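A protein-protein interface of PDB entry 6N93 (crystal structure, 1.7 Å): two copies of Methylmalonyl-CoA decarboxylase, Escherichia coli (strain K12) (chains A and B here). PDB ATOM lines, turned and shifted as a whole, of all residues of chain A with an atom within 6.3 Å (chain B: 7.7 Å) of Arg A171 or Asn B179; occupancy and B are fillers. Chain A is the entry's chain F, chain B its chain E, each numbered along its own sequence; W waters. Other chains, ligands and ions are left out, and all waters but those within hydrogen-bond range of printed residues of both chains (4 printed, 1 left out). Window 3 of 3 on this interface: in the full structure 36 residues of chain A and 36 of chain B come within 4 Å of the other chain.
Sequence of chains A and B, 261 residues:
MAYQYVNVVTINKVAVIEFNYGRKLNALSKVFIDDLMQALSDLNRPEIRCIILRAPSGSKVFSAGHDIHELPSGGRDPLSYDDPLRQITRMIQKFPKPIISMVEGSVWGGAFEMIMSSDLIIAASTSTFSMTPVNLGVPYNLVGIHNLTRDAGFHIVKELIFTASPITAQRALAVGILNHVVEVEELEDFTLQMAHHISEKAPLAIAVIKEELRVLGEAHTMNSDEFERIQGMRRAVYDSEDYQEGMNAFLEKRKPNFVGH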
ATOM      1  N   PHE A 154     -10.776 -17.011   3.364  1.00  0.00           N
ATOM      2  CA  PHE A 154     -12.225 -16.869   3.575  1.00  0.00           C
ATOM      3  C   PHE A 154     -12.941 -18.183   3.252  1.00  0.00           C
ATOM      4  O   PHE A 154     -13.847 -18.576   3.962  1.00  0.00           O
ATOM      5  CB  PHE A 154     -12.765 -15.766   2.669  1.00  0.00           C
ATOM      6  CG  PHE A 154     -13.202 -14.515   3.356  1.00  0.00           C
ATOM      7  CD1 PHE A 154     -12.468 -13.984   4.402  1.00  0.00           C
ATOM      8  CD2 PHE A 154     -14.298 -13.822   2.870  1.00  0.00           C
ATOM      9  CE1 PHE A 154     -12.906 -12.854   5.069  1.00  0.00           C
ATOM     10  CE2 PHE A 154     -14.685 -12.653   3.494  1.00  0.00           C
ATOM     11  CZ  PHE A 154     -13.997 -12.187   4.595  1.00  0.00           C
ATOM     12  N   HIS A 155     -12.668 -18.821   2.118  1.00  0.00           N
ATOM     13  CA  HIS A 155     -13.389 -20.082   1.796  1.00  0.00           C
ATOM     14  C   HIS A 155     -13.185 -21.105   2.921  1.00  0.00           C
ATOM     15  O   HIS A 155     -14.153 -21.828   3.293  1.00  0.00           O
ATOM     16  CB  HIS A 155     -12.920 -20.664   0.468  1.00  0.00           C
ATOM     17  CG  HIS A 155     -13.188 -19.797  -0.711  1.00  0.00           C
ATOM     18  ND1 HIS A 155     -12.466 -19.918  -1.874  1.00  0.00           N
ATOM     19  CD2 HIS A 155     -14.048 -18.763  -0.897  1.00  0.00           C
ATOM     20  CE1 HIS A 155     -12.876 -19.019  -2.749  1.00  0.00           C
ATOM     21  NE2 HIS A 155     -13.877 -18.302  -2.168  1.00  0.00           N
ATOM     22  N   ILE A 156     -11.981 -21.221   3.451  1.00  0.00           N
ATOM     23  CA  ILE A 156     -11.688 -22.201   4.538  1.00  0.00           C
ATOM     24  C   ILE A 156     -12.468 -21.811   5.792  1.00  0.00           C
ATOM     25  O   ILE A 156     -13.065 -22.687   6.443  1.00  0.00           O
ATOM     26  CB  ILE A 156     -10.186 -22.320   4.842  1.00  0.00           C
ATOM     27  CG1 ILE A 156      -9.392 -22.645   3.582  1.00  0.00           C
ATOM     28  CG2 ILE A 156      -9.974 -23.366   5.927  1.00  0.00           C
ATOM     29  CD1 ILE A 156      -9.814 -23.924   2.907  1.00  0.00           C
ATOM     30  N   VAL A 157     -12.429 -20.554   6.176  1.00  0.00           N
ATOM     31  CA  VAL A 157     -13.130 -20.121   7.405  1.00  0.00           C
ATOM     32  C   VAL A 157     -14.631 -20.399   7.234  1.00  0.00           C
ATOM     33  O   VAL A 157     -15.305 -20.861   8.182  1.00  0.00           O
ATOM     34  CB  VAL A 157     -12.821 -18.635   7.671  1.00  0.00           C
ATOM     35  CG1 VAL A 157     -13.746 -18.067   8.711  1.00  0.00           C
ATOM     36  CG2 VAL A 157     -11.353 -18.490   8.068  1.00  0.00           C
ATOM     37  N   LYS A 158     -15.181 -20.094   6.066  1.00  0.00           N
ATOM     38  CA  LYS A 158     -16.612 -20.352   5.832  1.00  0.00           C
ATOM     39  C   LYS A 158     -16.933 -21.845   5.942  1.00  0.00           C
ATOM     40  O   LYS A 158     -17.997 -22.149   6.486  1.00  0.00           O
ATOM     41  CB  LYS A 158     -17.072 -19.698   4.533  1.00  0.00           C
ATOM     42  CG  LYS A 158     -17.118 -18.170   4.625  1.00  0.00           C
ATOM     43  CD  LYS A 158     -17.222 -17.613   3.173  1.00  0.00           C
ATOM     44  CE  LYS A 158     -17.280 -16.142   3.027  1.00  0.00           C
ATOM     45  NZ  LYS A 158     -17.757 -15.781   1.675  1.00  0.00           N
ATOM     46  N   GLU A 159     -16.127 -22.726   5.367  1.00  0.00           N
ATOM     47  CA  GLU A 159     -16.345 -24.188   5.543  1.00  0.00           C
ATOM     48  C   GLU A 159     -16.357 -24.511   7.045  1.00  0.00           C
ATOM     49  O   GLU A 159     -17.303 -25.210   7.502  1.00  0.00           O
ATOM     50  CB  GLU A 159     -15.297 -24.996   4.808  1.00  0.00           C
ATOM     51  CG  GLU A 159     -15.446 -26.501   5.007  1.00  0.00           C
ATOM     52  CD  GLU A 159     -14.316 -27.323   4.398  1.00  0.00           C
ATOM     53  OE1 GLU A 159     -13.484 -26.777   3.618  1.00  0.00           O
ATOM     54  OE2 GLU A 159     -14.214 -28.500   4.784  1.00  0.00           O
ATOM     55  N   LEU A 160     -15.360 -24.057   7.808  1.00  0.00           N
ATOM     56  CA  LEU A 160     -15.310 -24.362   9.254  1.00  0.00           C
ATOM     57  C   LEU A 160     -16.609 -23.929   9.955  1.00  0.00           C
ATOM     58  O   LEU A 160     -17.185 -24.711  10.744  1.00  0.00           O
ATOM     59  CB  LEU A 160     -14.134 -23.612   9.877  1.00  0.00           C
ATOM     60  CG  LEU A 160     -12.767 -24.222   9.621  1.00  0.00           C
ATOM     61  CD1 LEU A 160     -11.693 -23.268  10.133  1.00  0.00           C
ATOM     62  CD2 LEU A 160     -12.659 -25.560  10.356  1.00  0.00           C
ATOM     63  N   PRO A 166     -15.219 -30.833  12.725  1.00  0.00           N
ATOM     64  CA  PRO A 166     -13.851 -30.809  13.207  1.00  0.00           C
ATOM     65  C   PRO A 166     -12.867 -30.985  12.062  1.00  0.00           C
ATOM     66  O   PRO A 166     -13.129 -31.733  11.088  1.00  0.00           O
ATOM     67  CB  PRO A 166     -13.751 -32.000  14.180  1.00  0.00           C
ATOM     68  CG  PRO A 166     -14.869 -32.907  13.798  1.00  0.00           C
ATOM     69  CD  PRO A 166     -15.945 -31.997  13.234  1.00  0.00           C
ATOM     70  N   ILE A 167     -11.764 -30.276  12.161  1.00  0.00           N
ATOM     71  CA  ILE A 167     -10.600 -30.545  11.279  1.00  0.00           C
ATOM     72  C   ILE A 167      -9.459 -31.129  12.110  1.00  0.00           C
ATOM     73  O   ILE A 167      -9.355 -30.833  13.337  1.00  0.00           O
ATOM     74  CB  ILE A 167     -10.194 -29.310  10.480  1.00  0.00           C
ATOM     75  CG1 ILE A 167      -9.654 -28.189  11.356  1.00  0.00           C
ATOM     76  CG2 ILE A 167     -11.358 -28.849   9.612  1.00  0.00           C
ATOM     77  CD1 ILE A 167      -8.942 -27.120  10.581  1.00  0.00           C
ATOM     78  N   THR A 168      -8.605 -31.889  11.437  1.00  0.00           N
ATOM     79  CA  THR A 168      -7.398 -32.480  12.062  1.00  0.00           C
ATOM     80  C   THR A 168      -6.352 -31.384  12.273  1.00  0.00           C
ATOM     81  O   THR A 168      -6.373 -30.366  11.628  1.00  0.00           O
ATOM     82  CB  THR A 168      -6.831 -33.604  11.202  1.00  0.00           C
ATOM     83  OG1 THR A 168      -6.435 -33.092   9.944  1.00  0.00           O
ATOM     84  CG2 THR A 168      -7.829 -34.725  11.011  1.00  0.00           C
ATOM     85  N   ALA A 169      -5.381 -31.675  13.126  1.00  0.00           N
ATOM     86  CA  ALA A 169      -4.154 -30.874  13.267  1.00  0.00           C
ATOM     87  C   ALA A 169      -3.415 -30.751  11.935  1.00  0.00           C
ATOM     88  O   ALA A 169      -2.913 -29.641  11.642  1.00  0.00           O
ATOM     89  CB  ALA A 169      -3.315 -31.509  14.352  1.00  0.00           C
ATOM     90  N   GLN A 170      -3.386 -31.807  11.106  1.00  0.00           N
ATOM     91  CA  GLN A 170      -2.650 -31.794   9.830  1.00  0.00           C
ATOM     92  C   GLN A 170      -3.325 -30.786   8.895  1.00  0.00           C
ATOM     93  O   GLN A 170      -2.623 -29.980   8.238  1.00  0.00           O
ATOM     94  CB  GLN A 170      -2.609 -33.207   9.234  1.00  0.00           C
ATOM     95  CG  GLN A 170      -1.739 -34.168  10.038  1.00  0.00           C
ATOM     96  CD  GLN A 170      -2.368 -34.625  11.330  1.00  0.00           C
ATOM     97  OE1 GLN A 170      -3.599 -34.676  11.472  1.00  0.00           O
ATOM     98  NE2 GLN A 170      -1.516 -34.941  12.307  1.00  0.00           N
ATOM     99  N   ARG A 171      -4.645 -30.804   8.866  1.00  0.00           N
ATOM    100  CA  ARG A 171      -5.360 -29.852   7.965  1.00  0.00           C
ATOM    101  C   ARG A 171      -5.255 -28.422   8.533  1.00  0.00           C
ATOM    102  O   ARG A 171      -5.034 -27.468   7.721  1.00  0.00           O
ATOM    103  CB  ARG A 171      -6.816 -30.213   7.726  1.00  0.00           C
ATOM    104  CG  ARG A 171      -7.430 -29.311   6.664  1.00  0.00           C
ATOM    105  CD  ARG A 171      -8.811 -29.706   6.252  1.00  0.00           C
ATOM    106  NE  ARG A 171      -9.235 -28.851   5.143  1.00  0.00           N
ATOM    107  CZ  ARG A 171     -10.488 -28.551   4.908  1.00  0.00           C
ATOM    108  NH1 ARG A 171     -11.425 -29.036   5.696  1.00  0.00           N
ATOM    109  NH2 ARG A 171     -10.805 -27.759   3.895  1.00  0.00           N
ATOM    110  N   ALA A 172      -5.404 -28.249   9.846  1.00  0.00           N
ATOM    111  CA  ALA A 172      -5.188 -26.913  10.457  1.00  0.00           C
ATOM    112  C   ALA A 172      -3.807 -26.354  10.088  1.00  0.00           C
ATOM    113  O   ALA A 172      -3.655 -25.108   9.870  1.00  0.00           O
ATOM    114  CB  ALA A 172      -5.388 -27.019  11.924  1.00  0.00           C
ATOM    115  N   LEU A 173      -2.771 -27.201  10.079  1.00  0.00           N
ATOM    116  CA  LEU A 173      -1.402 -26.789   9.674  1.00  0.00           C
ATOM    117  C   LEU A 173      -1.403 -26.375   8.192  1.00  0.00           C
ATOM    118  O   LEU A 173      -0.881 -25.295   7.871  1.00  0.00           O
ATOM    119  CB  LEU A 173      -0.416 -27.923   9.965  1.00  0.00           C
ATOM    120  CG  LEU A 173       1.038 -27.592   9.619  1.00  0.00           C
ATOM    121  CD1 LEU A 173       1.589 -26.563  10.603  1.00  0.00           C
ATOM    122  CD2 LEU A 173       1.897 -28.837   9.609  1.00  0.00           C
ATOM    123  N   ALA A 174      -1.967 -27.205   7.316  1.00  0.00           N
ATOM    124  CA  ALA A 174      -1.988 -26.992   5.858  1.00  0.00           C
ATOM    125  C   ALA A 174      -2.660 -25.638   5.515  1.00  0.00           C
ATOM    126  O   ALA A 174      -2.124 -24.900   4.663  1.00  0.00           O
ATOM    127  CB  ALA A 174      -2.671 -28.173   5.204  1.00  0.00           C
ATOM    128  N   VAL A 175      -3.744 -25.266   6.211  1.00  0.00           N
ATOM    129  CA  VAL A 175      -4.549 -24.062   5.811  1.00  0.00           C
ATOM    130  C   VAL A 175      -4.032 -22.803   6.512  1.00  0.00           C
ATOM    131  O   VAL A 175      -4.566 -21.740   6.226  1.00  0.00           O
ATOM    132  CB  VAL A 175      -6.058 -24.291   6.037  1.00  0.00           C
ATOM    133  CG1 VAL A 175      -6.588 -25.515   5.282  1.00  0.00           C
ATOM    134  CG2 VAL A 175      -6.418 -24.389   7.515  1.00  0.00           C
ATOM    135  N   GLY A 176      -3.074 -22.917   7.446  1.00  0.00           N
ATOM    136  CA  GLY A 176      -2.373 -21.767   8.060  1.00  0.00           C
ATOM    137  C   GLY A 176      -2.836 -21.407   9.468  1.00  0.00           C
ATOM    138  O   GLY A 176      -2.356 -20.385   9.996  1.00  0.00           O
ATOM    139  N   ILE A 177      -3.681 -22.215  10.106  1.00  0.00           N
ATOM    140  CA  ILE A 177      -4.158 -21.975  11.492  1.00  0.00           C
ATOM    141  C   ILE A 177      -3.026 -22.246  12.496  1.00  0.00           C
ATOM    142  O   ILE A 177      -2.848 -21.427  13.385  1.00  0.00           O
ATOM    143  CB  ILE A 177      -5.421 -22.804  11.755  1.00  0.00           C
ATOM    144  CG1 ILE A 177      -6.579 -22.185  10.973  1.00  0.00           C
ATOM    145  CG2 ILE A 177      -5.742 -22.911  13.223  1.00  0.00           C
ATOM    146  CD1 ILE A 177      -7.702 -23.155  10.764  1.00  0.00           C
ATOM    147  N   ILE B 100     -22.052 -22.903  -2.802  1.00  0.00           N
ATOM    148  CA  ILE B 100     -20.860 -23.750  -3.106  1.00  0.00           C
ATOM    149  C   ILE B 100     -20.678 -23.805  -4.613  1.00  0.00           C
ATOM    150  O   ILE B 100     -21.622 -24.228  -5.334  1.00  0.00           O
ATOM    151  CB  ILE B 100     -21.002 -25.164  -2.499  1.00  0.00           C
ATOM    152  CG1 ILE B 100     -21.303 -25.096  -1.004  1.00  0.00           C
ATOM    153  CG2 ILE B 100     -19.785 -26.032  -2.831  1.00  0.00           C
ATOM    154  CD1 ILE B 100     -21.668 -26.407  -0.393  1.00  0.00           C
ATOM    155  N   SER B 101     -19.483 -23.457  -5.100  1.00  0.00           N
ATOM    156  CA  SER B 101     -19.123 -23.682  -6.506  1.00  0.00           C
ATOM    157  C   SER B 101     -18.579 -25.107  -6.605  1.00  0.00           C
ATOM    158  O   SER B 101     -17.561 -25.423  -5.917  1.00  0.00           O
ATOM    159  CB  SER B 101     -18.135 -22.619  -6.978  1.00  0.00           C
ATOM    160  OG  SER B 101     -18.795 -21.364  -7.052  1.00  0.00           O
ATOM    161  N   SER B 118     -18.016 -16.860  -4.308  1.00  0.00           N
ATOM    162  CA  SER B 118     -18.872 -17.846  -3.635  1.00  0.00           C
ATOM    163  C   SER B 118     -18.207 -18.262  -2.323  1.00  0.00           C
ATOM    164  O   SER B 118     -17.068 -17.835  -2.047  1.00  0.00           O
ATOM    165  CB  SER B 118     -19.226 -19.016  -4.565  1.00  0.00           C
ATOM    166  OG  SER B 118     -18.159 -19.949  -4.735  1.00  0.00           O
ATOM    167  N   ASP B 119     -18.917 -19.035  -1.506  1.00  0.00           N
ATOM    168  CA  ASP B 119     -18.541 -19.288  -0.092  1.00  0.00           C
ATOM    169  C   ASP B 119     -17.520 -20.427   0.002  1.00  0.00           C
ATOM    170  O   ASP B 119     -16.599 -20.348   0.861  1.00  0.00           O
ATOM    171  CB  ASP B 119     -19.785 -19.519   0.733  1.00  0.00           C
ATOM    172  CG  ASP B 119     -20.694 -18.294   0.707  1.00  0.00           C
ATOM    173  OD1 ASP B 119     -20.172 -17.145   0.968  1.00  0.00           O
ATOM    174  OD2 ASP B 119     -21.875 -18.462   0.309  1.00  0.00           O
ATOM    175  N   LEU B 120     -17.680 -21.491  -0.800  1.00  0.00           N
ATOM    176  CA  LEU B 120     -16.776 -22.666  -0.768  1.00  0.00           C
ATOM    177  C   LEU B 120     -16.606 -23.109  -2.212  1.00  0.00           C
ATOM    178  O   LEU B 120     -17.541 -22.882  -3.057  1.00  0.00           O
ATOM    179  CB  LEU B 120     -17.391 -23.850   0.002  1.00  0.00           C
ATOM    180  CG  LEU B 120     -17.415 -23.890   1.526  1.00  0.00           C
ATOM    181  CD1 LEU B 120     -18.501 -23.034   2.099  1.00  0.00           C
ATOM    182  CD2 LEU B 120     -17.649 -25.329   2.011  1.00  0.00           C
ATOM    183  N   ILE B 121     -15.435 -23.632  -2.534  1.00  0.00           N
ATOM    184  CA  ILE B 121     -15.152 -24.207  -3.863  1.00  0.00           C
ATOM    185  C   ILE B 121     -14.682 -25.656  -3.676  1.00  0.00           C
ATOM    186  O   ILE B 121     -13.724 -25.899  -2.973  1.00  0.00           O
ATOM    187  CB  ILE B 121     -14.150 -23.410  -4.699  1.00  0.00           C
ATOM    188  CG1 ILE B 121     -14.445 -21.907  -4.721  1.00  0.00           C
ATOM    189  CG2 ILE B 121     -14.151 -23.985  -6.106  1.00  0.00           C
ATOM    190  CD1 ILE B 121     -13.306 -21.071  -5.314  1.00  0.00           C
ATOM    191  N   ILE B 122     -15.367 -26.601  -4.301  1.00  0.00           N
ATOM    192  CA  ILE B 122     -14.997 -28.042  -4.295  1.00  0.00           C
ATOM    193  C   ILE B 122     -14.813 -28.416  -5.769  1.00  0.00           C
ATOM    194  O   ILE B 122     -15.704 -28.087  -6.600  1.00  0.00           O
ATOM    195  CB  ILE B 122     -16.096 -28.866  -3.592  1.00  0.00           C
ATOM    196  CG1 ILE B 122     -16.281 -28.460  -2.130  1.00  0.00           C
ATOM    197  CG2 ILE B 122     -15.809 -30.341  -3.757  1.00  0.00           C
ATOM    198  CD1 ILE B 122     -17.461 -29.079  -1.441  1.00  0.00           C
ATOM    199  N   ALA B 123     -13.645 -28.941  -6.134  1.00  0.00           N
ATOM    200  CA  ALA B 123     -13.273 -29.099  -7.541  1.00  0.00           C
ATOM    201  C   ALA B 123     -12.832 -30.522  -7.858  1.00  0.00           C
ATOM    202  O   ALA B 123     -12.210 -31.171  -7.024  1.00  0.00           O
ATOM    203  CB  ALA B 123     -12.202 -28.124  -7.909  1.00  0.00           C
ATOM    204  N   ASP B 151      -8.197 -15.252  -0.274  1.00  0.00           N
ATOM    205  CA  ASP B 151      -7.919 -16.697  -0.058  1.00  0.00           C
ATOM    206  C   ASP B 151      -6.407 -16.951  -0.173  1.00  0.00           C
ATOM    207  O   ASP B 151      -5.811 -17.346   0.843  1.00  0.00           O
ATOM    208  CB  ASP B 151      -8.818 -17.468  -1.022  1.00  0.00           C
ATOM    209  CG  ASP B 151     -10.289 -17.291  -0.676  1.00  0.00           C
ATOM    210  OD1 ASP B 151     -10.717 -17.927   0.319  1.00  0.00           O
ATOM    211  OD2 ASP B 151     -10.981 -16.472  -1.388  1.00  0.00           O
ATOM    212  N   ALA B 172      -4.193 -24.902  -6.724  1.00  0.00           N
ATOM    213  CA  ALA B 172      -5.296 -24.079  -6.188  1.00  0.00           C
ATOM    214  C   ALA B 172      -5.620 -24.487  -4.747  1.00  0.00           C
ATOM    215  O   ALA B 172      -5.876 -23.595  -3.916  1.00  0.00           O
ATOM    216  CB  ALA B 172      -6.498 -24.141  -7.085  1.00  0.00           C
ATOM    217  N   LEU B 173      -5.614 -25.785  -4.427  1.00  0.00           N
ATOM    218  CA  LEU B 173      -5.809 -26.269  -3.048  1.00  0.00           C
ATOM    219  C   LEU B 173      -4.641 -25.805  -2.168  1.00  0.00           C
ATOM    220  O   LEU B 173      -4.888 -25.350  -1.016  1.00  0.00           O
ATOM    221  CB  LEU B 173      -5.950 -27.796  -3.018  1.00  0.00           C
ATOM    222  CG  LEU B 173      -6.234 -28.418  -1.659  1.00  0.00           C
ATOM    223  CD1 LEU B 173      -7.643 -28.146  -1.182  1.00  0.00           C
ATOM    224  CD2 LEU B 173      -6.022 -29.926  -1.708  1.00  0.00           C
ATOM    225  N   GLY B 176      -4.725 -22.103  -1.125  1.00  0.00           N
ATOM    226  CA  GLY B 176      -5.893 -21.744  -0.316  1.00  0.00           C
ATOM    227  C   GLY B 176      -7.104 -21.279  -1.098  1.00  0.00           C
ATOM    228  O   GLY B 176      -8.049 -20.819  -0.455  1.00  0.00           O
ATOM    229  N   ILE B 177      -7.109 -21.370  -2.427  1.00  0.00           N
ATOM    230  CA  ILE B 177      -8.260 -20.985  -3.274  1.00  0.00           C
ATOM    231  C   ILE B 177      -9.382 -22.015  -3.066  1.00  0.00           C
ATOM    232  O   ILE B 177     -10.576 -21.607  -2.903  1.00  0.00           O
ATOM    233  CB  ILE B 177      -7.794 -20.846  -4.729  1.00  0.00           C
ATOM    234  CG1 ILE B 177      -6.937 -19.588  -4.879  1.00  0.00           C
ATOM    235  CG2 ILE B 177      -8.962 -20.880  -5.693  1.00  0.00           C
ATOM    236  CD1 ILE B 177      -6.135 -19.528  -6.132  1.00  0.00           C
ATOM    237  N   LEU B 178      -9.048 -23.295  -3.048  1.00  0.00           N
ATOM    238  CA  LEU B 178     -10.057 -24.375  -2.996  1.00  0.00           C
ATOM    239  C   LEU B 178     -10.234 -24.921  -1.582  1.00  0.00           C
ATOM    240  O   LEU B 178      -9.273 -24.980  -0.817  1.00  0.00           O
ATOM    241  CB  LEU B 178      -9.659 -25.519  -3.941  1.00  0.00           C
ATOM    242  CG  LEU B 178      -9.522 -25.179  -5.412  1.00  0.00           C
ATOM    243  CD1 LEU B 178      -9.108 -26.402  -6.194  1.00  0.00           C
ATOM    244  CD2 LEU B 178     -10.783 -24.603  -6.004  1.00  0.00           C
ATOM    245  N   ASN B 179     -11.415 -25.438  -1.285  1.00  0.00           N
ATOM    246  CA  ASN B 179     -11.698 -26.156  -0.031  1.00  0.00           C
ATOM    247  C   ASN B 179     -11.259 -27.606  -0.149  1.00  0.00           C
ATOM    248  O   ASN B 179     -10.613 -28.111   0.787  1.00  0.00           O
ATOM    249  CB  ASN B 179     -13.171 -26.090   0.318  1.00  0.00           C
ATOM    250  CG  ASN B 179     -13.567 -24.693   0.729  1.00  0.00           C
ATOM    251  OD1 ASN B 179     -13.834 -23.855  -0.172  1.00  0.00           O
ATOM    252  ND2 ASN B 179     -13.582 -24.446   2.046  1.00  0.00           N
ATOM    253  N   HIS B 180     -11.698 -28.256  -1.231  1.00  0.00           N
ATOM    254  CA  HIS B 180     -11.496 -29.707  -1.461  1.00  0.00           C
ATOM    255  C   HIS B 180     -11.263 -29.983  -2.935  1.00  0.00           C
ATOM    256  O   HIS B 180     -11.852 -29.302  -3.818  1.00  0.00           O
ATOM    257  CB  HIS B 180     -12.646 -30.529  -0.902  1.00  0.00           C
ATOM    258  CG  HIS B 180     -12.788 -30.451   0.578  1.00  0.00           C
ATOM    259  ND1 HIS B 180     -11.994 -31.208   1.444  1.00  0.00           N
ATOM    260  CD2 HIS B 180     -13.602 -29.696   1.349  1.00  0.00           C
ATOM    261  CE1 HIS B 180     -12.390 -30.966   2.682  1.00  0.00           C
ATOM    262  NE2 HIS B 180     -13.348 -30.017   2.658  1.00  0.00           N
ATOM    263  N   VAL B 181     -10.415 -30.968  -3.167  1.00  0.00           N
ATOM    264  CA  VAL B 181     -10.183 -31.550  -4.503  1.00  0.00           C
ATOM    265  C   VAL B 181     -10.599 -33.016  -4.412  1.00  0.00           C
ATOM    266  O   VAL B 181     -10.172 -33.683  -3.489  1.00  0.00           O
ATOM    267  CB  VAL B 181      -8.731 -31.369  -4.980  1.00  0.00           C
ATOM    268  CG1 VAL B 181      -8.509 -32.125  -6.284  1.00  0.00           C
ATOM    269  CG2 VAL B 181      -8.380 -29.879  -5.124  1.00  0.00           C
ATOM    270  N   PHE B 190     -19.815 -36.030  -2.975  1.00  0.00           N
ATOM    271  CA  PHE B 190     -19.029 -35.367  -1.903  1.00  0.00           C
ATOM    272  C   PHE B 190     -19.653 -34.002  -1.587  1.00  0.00           C
ATOM    273  O   PHE B 190     -19.851 -33.691  -0.390  1.00  0.00           O
ATOM    274  CB  PHE B 190     -17.573 -35.209  -2.352  1.00  0.00           C
ATOM    275  CG  PHE B 190     -16.701 -34.600  -1.291  1.00  0.00           C
ATOM    276  CD1 PHE B 190     -16.569 -33.219  -1.208  1.00  0.00           C
ATOM    277  CD2 PHE B 190     -16.019 -35.394  -0.380  1.00  0.00           C
ATOM    278  CE1 PHE B 190     -15.808 -32.636  -0.205  1.00  0.00           C
ATOM    279  CE2 PHE B 190     -15.267 -34.799   0.634  1.00  0.00           C
ATOM    280  CZ  PHE B 190     -15.144 -33.416   0.696  1.00  0.00           C
ATOM    281  N   MET B 194     -21.885 -32.641   1.860  1.00  0.00           N
ATOM    282  CA  MET B 194     -21.528 -31.409   2.627  1.00  0.00           C
ATOM    283  C   MET B 194     -22.695 -30.403   2.646  1.00  0.00           C
ATOM    284  O   MET B 194     -22.968 -29.823   3.706  1.00  0.00           O
ATOM    285  CB  MET B 194     -20.254 -30.743   2.084  1.00  0.00           C
ATOM    286  CG  MET B 194     -19.745 -29.689   3.080  1.00  0.00           C
ATOM    287  SD  MET B 194     -18.205 -28.996   2.553  1.00  0.00           S
ATOM    288  CE  MET B 194     -17.087 -30.307   3.005  1.00  0.00           C
HETATM  289  O   HOH W   1     -16.043 -15.876  -0.399  1.00  0.00           O
HETATM  290  O   HOH W   2      -9.675 -20.025   1.660  1.00  0.00           O
HETATM  291  O   HOH W   3     -13.452 -15.359  -0.793  1.00  0.00           O
HETATM  292  O   HOH W   4     -19.997 -15.170  -0.605  1.00  0.00           O
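OG of Ser B101 lies within hydrogen-bond range of OG of Ser B118, 2.8 Å away.
O of Leu B120 lies within hydrogen-bond range of N of Ser B101 (2.9 Å).
The side-chain hydroxyl (OG) of Ser B118 lies within hydrogen-bond range of the backbone carbonyl oxygen (O) of Leu B120, at 3.4 Å.
The backbone NH (N) of Ile B121 is in hydrogen-bond range of the side-chain amide oxygen (OD1) of Asn B179 (2.9 Å).
The backbone NH (N) of Ala B123 is in hydrogen-bond range of the backbone carbonyl oxygen (O) of His B180 (3.0 Å).
N of Leu B178 sits at hydrogen-bond distance from O of Ala B172, 3.3 Å away.
The backbone carbonyl oxygen (O) of Ser B118 sits at hydrogen-bond distance from a ring nitrogen (NE2) of His A155 (3.2 Å).
OD1 of Asp B119 lies within salt-bridge range of NZ of Lys A158 (2.9 Å).
The side-chain carboxylate (OD1) of Asp B151 is in hydrogen-bond range of the backbone NH (N) of Phe A154, 3.2 Å away.
OD1 of Asp B151 sits at hydrogen-bond distance from N of His A155 (2.8 Å).
The backbone carbonyl oxygen of Ile B177 lies within hydrogen-bond range of a ring nitrogen (ND1) of His A155, at 2.7 Å.
ND2 of Asn B179 is in hydrogen-bond range of O of His A155, 3.0 Å away.
The side-chain carboxylate (OE1) of Glu A159 lies within hydrogen-bond range of the side-chain amide nitrogen (ND2) of Asn B179 (2.8 Å).
The guanidinium group (NH2) of Arg A171 is in hydrogen-bond range of the backbone carbonyl oxygen (O) of Asn B179 (3.1 Å).
The side-chain carboxylate of Glu A159 sits at hydrogen-bond distance from a ring nitrogen (NE2) of His B180, 2.8 Å away.
Hydrophobic or aromatic side chains of chain B within 4 Å of the printed part of chain A: Leu B120, Ile B121, His B180 and Met B194.
Printed residues of chain A that touch a printed residue of chain B: Phe A154, His A155, Ile A156, Lys A158, Glu A159 and Arg A171.
Hydrophobic or aromatic side chains of chain A within 4 Å of the printed part of chain B: Phe A154, His A155 and Ile A156.
Among the printed residues, 16 pairs touch across the chains.
Water W4 lies within hydrogen-bond range of OD1 of Asp B119 (2.5 Å) and NZ of Lys A158 (3.3 Å).
Water W1 bridges NZ of Lys A158 (2.7 Å) and O of Ser B118 (2.8 Å).
Water W2 lies within hydrogen-bond range of the side-chain carboxylate (OD1) of Asp B151, the backbone carbonyl oxygen (O) of Gly B176, the backbone NH (N) of Ile A156 and the backbone NH (N) of His A155.
Water W3 bridges OD2 of Asp B151 (2.8 Å) and NE2 of His A155 (3.3 Å).
4 positions are printed for both chains.
Among the printed residues, pairs that only touch across the chains: His A155 with Ile B121 (3.3 Å), His A155 with Asp B119 (3.4 Å), Arg A171 with His B180 (3.6 Å), Glu A159 with Leu B120 (3.7 Å), Glu A159 with Met B194 (3.8 Å), Ile A156 with Asn B179 (3.9 Å) and Ile A156 with Leu B178 (3.9 Å).
Of chain B, only Asn B179 and His B180 come within 4 Å of Arg A171.
Of the printed residues of chain A, Asn B179 touches His A155 (3.0 Å), Ile A156 (3.9 Å), Glu A159 (2.8 Å) and Arg A171 (3.1 Å).
Printed residues of chain B within 4 Å of Phe A154: Asp B151 (3.2 Å).
Printed residues of chain A within 4 Å of Asp B151: Phe A154 (3.2 Å) and His A155 (2.8 Å).
Of the printed residues of chain B, His A155 touches Ser B118, Asp B119, Ile B121, Asp B151, Ile B177 and Asn B179.
Printed residues of chain A within 4 Å of Leu B120: Glu A159 (3.7 Å).
Of the printed residues of chain B, Glu A159 touches Leu B120, Asn B179, His B180 and Met B194.
The nearest residue of chain B that does not touch Arg A171 is Leu B178 (5.7 Å).
The nearest printed residue of chain A that does not touch Asn B179 is Lys A158 (5.8 Å).
The nearest printed residue of chain B that does not touch Ile A156 is Gly B176 (4.6 Å).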
